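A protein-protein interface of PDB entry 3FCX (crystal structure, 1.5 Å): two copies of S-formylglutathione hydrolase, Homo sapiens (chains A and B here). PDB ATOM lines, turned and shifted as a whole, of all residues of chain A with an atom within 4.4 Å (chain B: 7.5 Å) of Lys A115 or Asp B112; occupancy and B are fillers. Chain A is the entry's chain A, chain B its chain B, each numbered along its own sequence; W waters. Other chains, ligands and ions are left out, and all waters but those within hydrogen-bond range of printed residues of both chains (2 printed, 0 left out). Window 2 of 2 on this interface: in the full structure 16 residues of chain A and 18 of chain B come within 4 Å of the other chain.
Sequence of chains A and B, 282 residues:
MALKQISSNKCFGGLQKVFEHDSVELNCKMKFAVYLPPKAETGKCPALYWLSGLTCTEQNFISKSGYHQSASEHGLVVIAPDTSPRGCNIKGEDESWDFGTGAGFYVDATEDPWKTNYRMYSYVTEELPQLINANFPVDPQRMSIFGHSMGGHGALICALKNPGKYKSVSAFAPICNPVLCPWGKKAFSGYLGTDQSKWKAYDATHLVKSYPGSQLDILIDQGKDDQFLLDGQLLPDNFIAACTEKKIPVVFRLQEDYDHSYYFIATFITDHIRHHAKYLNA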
ATOM      1  N   ALA A 109      22.877   6.139  -3.609  1.00  0.00           N
ATOM      2  CA  ALA A 109      22.706   4.821  -4.220  1.00  0.00           C
ATOM      3  C   ALA A 109      23.419   3.726  -3.433  1.00  0.00           C
ATOM      4  O   ALA A 109      24.496   3.945  -2.876  1.00  0.00           O
ATOM      5  CB  ALA A 109      23.181   4.843  -5.660  1.00  0.00           C
ATOM      6  N   THR A 110      22.799   2.549  -3.397  1.00  0.00           N
ATOM      7  CA  THR A 110      23.343   1.406  -2.670  1.00  0.00           C
ATOM      8  C   THR A 110      23.682   0.251  -3.609  1.00  0.00           C
ATOM      9  O   THR A 110      24.224  -0.759  -3.172  1.00  0.00           O
ATOM     10  CB  THR A 110      22.358   0.890  -1.607  1.00  0.00           C
ATOM     11  OG1 THR A 110      21.115   0.567  -2.236  1.00  0.00           O
ATOM     12  CG2 THR A 110      22.126   1.932  -0.521  1.00  0.00           C
ATOM     13  N   GLU A 111      23.358   0.403  -4.891  1.00  0.00           N
ATOM     14  CA  GLU A 111      23.658  -0.627  -5.885  1.00  0.00           C
ATOM     15  C   GLU A 111      24.768  -0.177  -6.819  1.00  0.00           C
ATOM     16  O   GLU A 111      24.784   0.967  -7.269  1.00  0.00           O
ATOM     17  CB  GLU A 111      22.417  -0.972  -6.712  1.00  0.00           C
ATOM     18  CG  GLU A 111      21.168  -1.261  -5.900  1.00  0.00           C
ATOM     19  CD  GLU A 111      21.346  -2.409  -4.924  1.00  0.00           C
ATOM     20  OE1 GLU A 111      21.439  -3.570  -5.376  1.00  0.00           O
ATOM     21  OE2 GLU A 111      21.390  -2.146  -3.704  1.00  0.00           O
ATOM     22  N   ASP A 112      25.698  -1.087  -7.106  1.00  0.00           N
ATOM     23  CA  ASP A 112      26.706  -0.851  -8.132  1.00  0.00           C
ATOM     24  C   ASP A 112      26.028  -0.900  -9.506  1.00  0.00           C
ATOM     25  O   ASP A 112      25.057  -1.638  -9.688  1.00  0.00           O
ATOM     26  CB  ASP A 112      27.834  -1.890  -8.043  1.00  0.00           C
ATOM     27  CG  ASP A 112      28.988  -1.441  -7.150  1.00  0.00           C
ATOM     28  OD1 ASP A 112      29.365  -0.248  -7.188  1.00  0.00           O
ATOM     29  OD2 ASP A 112      29.537  -2.293  -6.419  1.00  0.00           O
ATOM     30  N   PRO A 113      26.521  -0.100 -10.471  1.00  0.00           N
ATOM     31  CA  PRO A 113      27.666   0.804 -10.361  1.00  0.00           C
ATOM     32  C   PRO A 113      27.311   2.196  -9.825  1.00  0.00           C
ATOM     33  O   PRO A 113      28.206   3.016  -9.630  1.00  0.00           O
ATOM     34  CB  PRO A 113      28.160   0.903 -11.802  1.00  0.00           C
ATOM     35  CG  PRO A 113      26.931   0.749 -12.619  1.00  0.00           C
ATOM     36  CD  PRO A 113      25.956  -0.093 -11.834  1.00  0.00           C
ATOM     37  N   TRP A 114      26.024   2.448  -9.590  1.00  0.00           N
ATOM     38  CA  TRP A 114      25.562   3.748  -9.090  1.00  0.00           C
ATOM     39  C   TRP A 114      26.149   4.073  -7.714  1.00  0.00           C
ATOM     40  O   TRP A 114      26.430   5.235  -7.414  1.00  0.00           O
ATOM     41  CB  TRP A 114      24.032   3.789  -9.029  1.00  0.00           C
ATOM     42  CG  TRP A 114      23.339   3.382 -10.301  1.00  0.00           C
ATOM     43  CD1 TRP A 114      22.625   2.238 -10.512  1.00  0.00           C
ATOM     44  CD2 TRP A 114      23.289   4.119 -11.530  1.00  0.00           C
ATOM     45  NE1 TRP A 114      22.134   2.216 -11.795  1.00  0.00           N
ATOM     46  CE2 TRP A 114      22.526   3.357 -12.442  1.00  0.00           C
ATOM     47  CE3 TRP A 114      23.816   5.350 -11.949  1.00  0.00           C
ATOM     48  CZ2 TRP A 114      22.272   3.787 -13.749  1.00  0.00           C
ATOM     49  CZ3 TRP A 114      23.566   5.774 -13.252  1.00  0.00           C
ATOM     50  CH2 TRP A 114      22.801   4.992 -14.135  1.00  0.00           C
ATOM     51  N   LYS A 115      26.303   3.031  -6.894  1.00  0.00           N
ATOM     52  CA  LYS A 115      26.970   3.053  -5.583  1.00  0.00           C
ATOM     53  C   LYS A 115      28.148   4.008  -5.468  1.00  0.00           C
ATOM     54  O   LYS A 115      28.218   4.821  -4.540  1.00  0.00           O
ATOM     55  CB  LYS A 115      27.508   1.653  -5.286  1.00  0.00           C
ATOM     56  CG  LYS A 115      26.975   0.967  -4.056  1.00  0.00           C
ATOM     57  CD  LYS A 115      27.235  -0.531  -4.181  1.00  0.00           C
ATOM     58  CE  LYS A 115      27.486  -1.209  -2.850  1.00  0.00           C
ATOM     59  NZ  LYS A 115      26.431  -0.969  -1.823  1.00  0.00           N
ATOM     60  N   THR A 116      29.087   3.875  -6.400  1.00  0.00           N
ATOM     61  CA  THR A 116      30.385   4.532  -6.288  1.00  0.00           C
ATOM     62  C   THR A 116      30.312   6.055  -6.449  1.00  0.00           C
ATOM     63  O   THR A 116      31.080   6.780  -5.814  1.00  0.00           O
ATOM     64  CB  THR A 116      31.451   3.895  -7.240  1.00  0.00           C
ATOM     65  OG1 THR A 116      32.715   4.540  -7.055  1.00  0.00           O
ATOM     66  CG2 THR A 116      31.042   3.998  -8.704  1.00  0.00           C
ATOM     67  N   ASN A 117      29.371   6.528  -7.265  1.00  0.00           N
ATOM     68  CA  ASN A 117      29.328   7.939  -7.653  1.00  0.00           C
ATOM     69  C   ASN A 117      28.023   8.678  -7.375  1.00  0.00           C
ATOM     70  O   ASN A 117      28.040   9.883  -7.114  1.00  0.00           O
ATOM     71  CB  ASN A 117      29.698   8.083  -9.129  1.00  0.00           C
ATOM     72  CG  ASN A 117      31.045   7.468  -9.449  1.00  0.00           C
ATOM     73  OD1 ASN A 117      31.988   7.572  -8.659  1.00  0.00           O
ATOM     74  ND2 ASN A 117      31.145   6.825 -10.605  1.00  0.00           N
ATOM     75  N   ARG A 119      25.798   9.822  -5.174  1.00  0.00           N
ATOM     76  CA  ARG A 119      25.585  10.118  -3.759  1.00  0.00           C
ATOM     77  C   ARG A 119      24.964  11.502  -3.637  1.00  0.00           C
ATOM     78  O   ARG A 119      25.453  12.376  -2.907  1.00  0.00           O
ATOM     79  CB  ARG A 119      26.894  10.015  -2.962  1.00  0.00           C
ATOM     80  CG  ARG A 119      27.555   8.634  -2.985  1.00  0.00           C
ATOM     81  CD  ARG A 119      26.817   7.617  -2.126  1.00  0.00           C
ATOM     82  NE  ARG A 119      27.478   6.312  -2.142  1.00  0.00           N
ATOM     83  CZ  ARG A 119      28.445   5.942  -1.306  1.00  0.00           C
ATOM     84  NH1 ARG A 119      28.886   6.771  -0.366  1.00  0.00           N
ATOM     85  NH2 ARG A 119      28.979   4.731  -1.413  1.00  0.00           N
ATOM     86  N   ILE B  90      29.552  -9.587   8.797  1.00  0.00           N
ATOM     87  CA  ILE B  90      30.189  -8.687   7.838  1.00  0.00           C
ATOM     88  C   ILE B  90      31.695  -8.699   8.075  1.00  0.00           C
ATOM     89  O   ILE B  90      32.150  -8.610   9.214  1.00  0.00           O
ATOM     90  CB  ILE B  90      29.653  -7.243   7.970  1.00  0.00           C
ATOM     91  CG1 ILE B  90      28.138  -7.205   7.751  1.00  0.00           C
ATOM     92  CG2 ILE B  90      30.354  -6.314   6.981  1.00  0.00           C
ATOM     93  CD1 ILE B  90      27.464  -5.975   8.342  1.00  0.00           C
ATOM     94  N   ALA B 109      25.600   4.695   8.431  1.00  0.00           N
ATOM     95  CA  ALA B 109      26.823   4.557   7.647  1.00  0.00           C
ATOM     96  C   ALA B 109      26.556   4.755   6.156  1.00  0.00           C
ATOM     97  O   ALA B 109      25.512   4.340   5.640  1.00  0.00           O
ATOM     98  CB  ALA B 109      27.460   3.206   7.903  1.00  0.00           C
ATOM     99  N   THR B 110      27.506   5.403   5.487  1.00  0.00           N
ATOM    100  CA  THR B 110      27.406   5.706   4.062  1.00  0.00           C
ATOM    101  C   THR B 110      28.372   4.864   3.228  1.00  0.00           C
ATOM    102  O   THR B 110      28.236   4.790   2.006  1.00  0.00           O
ATOM    103  CB  THR B 110      27.680   7.202   3.783  1.00  0.00           C
ATOM    104  OG1 THR B 110      28.982   7.555   4.260  1.00  0.00           O
ATOM    105  CG2 THR B 110      26.630   8.080   4.461  1.00  0.00           C
ATOM    106  N   GLU B 111      29.337   4.233   3.894  1.00  0.00           N
ATOM    107  CA  GLU B 111      30.393   3.484   3.214  1.00  0.00           C
ATOM    108  C   GLU B 111      30.156   1.983   3.259  1.00  0.00           C
ATOM    109  O   GLU B 111      29.706   1.443   4.272  1.00  0.00           O
ATOM    110  CB  GLU B 111      31.757   3.798   3.836  1.00  0.00           C
ATOM    111  CG  GLU B 111      32.090   5.280   3.917  1.00  0.00           C
ATOM    112  CD  GLU B 111      31.981   5.989   2.581  1.00  0.00           C
ATOM    113  OE1 GLU B 111      32.876   5.787   1.732  1.00  0.00           O
ATOM    114  OE2 GLU B 111      31.005   6.752   2.385  1.00  0.00           O
ATOM    115  N   ASP B 112      30.457   1.316   2.146  1.00  0.00           N
ATOM    116  CA  ASP B 112      30.522  -0.140   2.113  1.00  0.00           C
ATOM    117  C   ASP B 112      31.658  -0.615   3.021  1.00  0.00           C
ATOM    118  O   ASP B 112      32.697   0.038   3.092  1.00  0.00           O
ATOM    119  CB  ASP B 112      30.771  -0.620   0.685  1.00  0.00           C
ATOM    120  CG  ASP B 112      29.569  -0.436  -0.206  1.00  0.00           C
ATOM    121  OD1 ASP B 112      28.552  -1.122   0.027  1.00  0.00           O
ATOM    122  OD2 ASP B 112      29.645   0.390  -1.143  1.00  0.00           O
ATOM    123  N   PRO B 113      31.475  -1.758   3.711  1.00  0.00           N
ATOM    124  CA  PRO B 113      30.341  -2.685   3.690  1.00  0.00           C
ATOM    125  C   PRO B 113      29.280  -2.391   4.756  1.00  0.00           C
ATOM    126  O   PRO B 113      28.466  -3.263   5.057  1.00  0.00           O
ATOM    127  CB  PRO B 113      31.012  -4.022   4.002  1.00  0.00           C
ATOM    128  CG  PRO B 113      32.083  -3.648   4.975  1.00  0.00           C
ATOM    129  CD  PRO B 113      32.569  -2.273   4.559  1.00  0.00           C
ATOM    130  N   TRP B 114      29.285  -1.175   5.298  1.00  0.00           N
ATOM    131  CA  TRP B 114      28.459  -0.832   6.463  1.00  0.00           C
ATOM    132  C   TRP B 114      27.090  -0.236   6.114  1.00  0.00           C
ATOM    133  O   TRP B 114      26.209  -0.159   6.976  1.00  0.00           O
ATOM    134  CB  TRP B 114      29.232   0.113   7.399  1.00  0.00           C
ATOM    135  CG  TRP B 114      30.700  -0.219   7.520  1.00  0.00           C
ATOM    136  CD1 TRP B 114      31.751   0.545   7.099  1.00  0.00           C
ATOM    137  CD2 TRP B 114      31.270  -1.414   8.074  1.00  0.00           C
ATOM    138  NE1 TRP B 114      32.940  -0.090   7.367  1.00  0.00           N
ATOM    139  CE2 TRP B 114      32.674  -1.295   7.965  1.00  0.00           C
ATOM    140  CE3 TRP B 114      30.732  -2.571   8.657  1.00  0.00           C
ATOM    141  CZ2 TRP B 114      33.549  -2.294   8.411  1.00  0.00           C
ATOM    142  CZ3 TRP B 114      31.603  -3.561   9.105  1.00  0.00           C
ATOM    143  CH2 TRP B 114      32.996  -3.414   8.979  1.00  0.00           C
ATOM    144  N   LYS B 115      26.915   0.163   4.854  1.00  0.00           N
ATOM    145  CA  LYS B 115      25.716   0.882   4.385  1.00  0.00           C
ATOM    146  C   LYS B 115      24.381   0.220   4.716  1.00  0.00           C
ATOM    147  O   LYS B 115      23.419   0.902   5.079  1.00  0.00           O
ATOM    148  CB  LYS B 115      25.764   1.073   2.865  1.00  0.00           C
ATOM    149  CG  LYS B 115      26.854   1.982   2.355  1.00  0.00           C
ATOM    150  CD  LYS B 115      26.847   2.073   0.826  1.00  0.00           C
ATOM    151  CE  LYS B 115      25.663   2.881   0.288  1.00  0.00           C
ATOM    152  NZ  LYS B 115      25.681   4.317   0.699  1.00  0.00           N
ATOM    153  N   THR B 116      24.318  -1.099   4.565  1.00  0.00           N
ATOM    154  CA  THR B 116      23.043  -1.817   4.627  1.00  0.00           C
ATOM    155  C   THR B 116      22.576  -2.134   6.049  1.00  0.00           C
ATOM    156  O   THR B 116      21.380  -2.067   6.332  1.00  0.00           O
ATOM    157  CB  THR B 116      23.045  -3.100   3.743  1.00  0.00           C
ATOM    158  OG1 THR B 116      21.838  -3.843   3.962  1.00  0.00           O
ATOM    159  CG2 THR B 116      24.246  -3.984   4.040  1.00  0.00           C
ATOM    160  N   GLY B 190      35.576   4.972   9.119  1.00  0.00           N
ATOM    161  CA  GLY B 190      35.084   3.678   8.668  1.00  0.00           C
ATOM    162  C   GLY B 190      33.681   3.761   8.104  1.00  0.00           C
ATOM    163  O   GLY B 190      33.429   3.317   6.981  1.00  0.00           O
ATOM    164  N   TYR B 191      32.773   4.357   8.875  1.00  0.00           N
ATOM    165  CA  TYR B 191      31.355   4.368   8.518  1.00  0.00           C
ATOM    166  C   TYR B 191      30.977   5.442   7.500  1.00  0.00           C
ATOM    167  O   TYR B 191      30.076   5.231   6.687  1.00  0.00           O
ATOM    168  CB  TYR B 191      30.478   4.561   9.760  1.00  0.00           C
ATOM    169  CG  TYR B 191      30.512   3.450  10.788  1.00  0.00           C
ATOM    170  CD1 TYR B 191      30.403   2.107  10.414  1.00  0.00           C
ATOM    171  CD2 TYR B 191      30.606   3.747  12.147  1.00  0.00           C
ATOM    172  CE1 TYR B 191      30.416   1.085  11.375  1.00  0.00           C
ATOM    173  CE2 TYR B 191      30.621   2.739  13.110  1.00  0.00           C
ATOM    174  CZ  TYR B 191      30.530   1.411  12.717  1.00  0.00           C
ATOM    175  OH  TYR B 191      30.546   0.416  13.671  1.00  0.00           O
HETATM  176  O   HOH W   1      30.866   8.828   0.361  1.00  0.00           O
HETATM  177  O   HOH W   2      31.651   3.009  -0.047  1.00  0.00           O
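The backbone carbonyl oxygen (O) of Tyr B191 sits at hydrogen-bond distance from the backbone NH (N) of Thr B110, 2.8 Å away.
The backbone NH (N) of Glu B111 is in hydrogen-bond range of the backbone carbonyl oxygen (O) of Tyr B191, 3.1 Å away.
The backbone carbonyl oxygen of Lys A115 sits at hydrogen-bond distance from the guanidinium group of Arg A119 (2.9 Å).
The side-chain hydroxyl (OG1) of Thr B110 sits at hydrogen-bond distance from the side-chain carboxylate (OE2) of Glu B111 (2.9 Å).
The backbone carbonyl oxygen of Thr B110 sits at hydrogen-bond distance from the side-chain amino group of Lys B115, 2.9 Å away.
O of Thr A110 is in hydrogen-bond range of NZ of Lys A115 (2.6 Å).
Ala A109 touches Lys B115, but with the chains exchanged Lys A115 does not touch Ala B109 (9.2 Å).
Thr A110 touches Lys B115, but with the chains exchanged Lys A115 does not touch Thr B110 (6.5 Å).
Lys A115 touches Asp B112, but with the chains exchanged Asp A112 does not touch Lys B115 (8.4 Å).
Positions printed for both chains: 109, 110, 111, 112, 113, 114, 115 and 116.
The backbone carbonyl oxygen (O) of Thr B110 lies within hydrogen-bond range of the guanidinium group (NH1) of Arg A119 (3.2 Å).
The side-chain carboxylate of Asp B112 is in salt-bridge range of the side-chain amino group of Lys A115, at 2.8 Å.
The guanidinium group (NH1) of Arg A119 lies within salt-bridge range of the side-chain carboxylate (OE2) of Glu B111 (3.5 Å).
Of the printed residues of chain B, Ala A109 touches Lys B115.
Printed residues of chain B within 4 Å of Lys A115: Asp B112 (2.8 Å).
Asp B112 touches one residue of chain A.
Printed residues of chain A within 4 Å of Lys B115: Ala A109, Thr A110 and Arg A119.
The nearest printed residue of chain A that does not touch Asp B112 is Arg A119 (4.4 Å).
The nearest printed residue of chain A that does not touch Glu B111 is Lys A115 (7.0 Å).
Among the printed residues, pairs that only touch across the chains: Ala A109 with Lys B115 (3.5 Å), Thr A110 with Lys B115 (3.8 Å) and Arg A119 with Lys B115 (3.8 Å).
Water W1 bridges OE2 of Glu B111 (2.9 Å) and NH1 of Arg A119 (2.9 Å).
Water W2 bridges the backbone NH of Asp B112 (3.0 Å) and the guanidinium group of Arg A119 (3.5 Å).
Along chain B the printed residues that touch a printed residue of chain A span positions 110 to 115.
Printed residues of chain A that touch a printed residue of chain B: Ala A109, Thr A110, Lys A115 and Arg A119.
Among the printed residues, 6 pairs touch across the chains.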
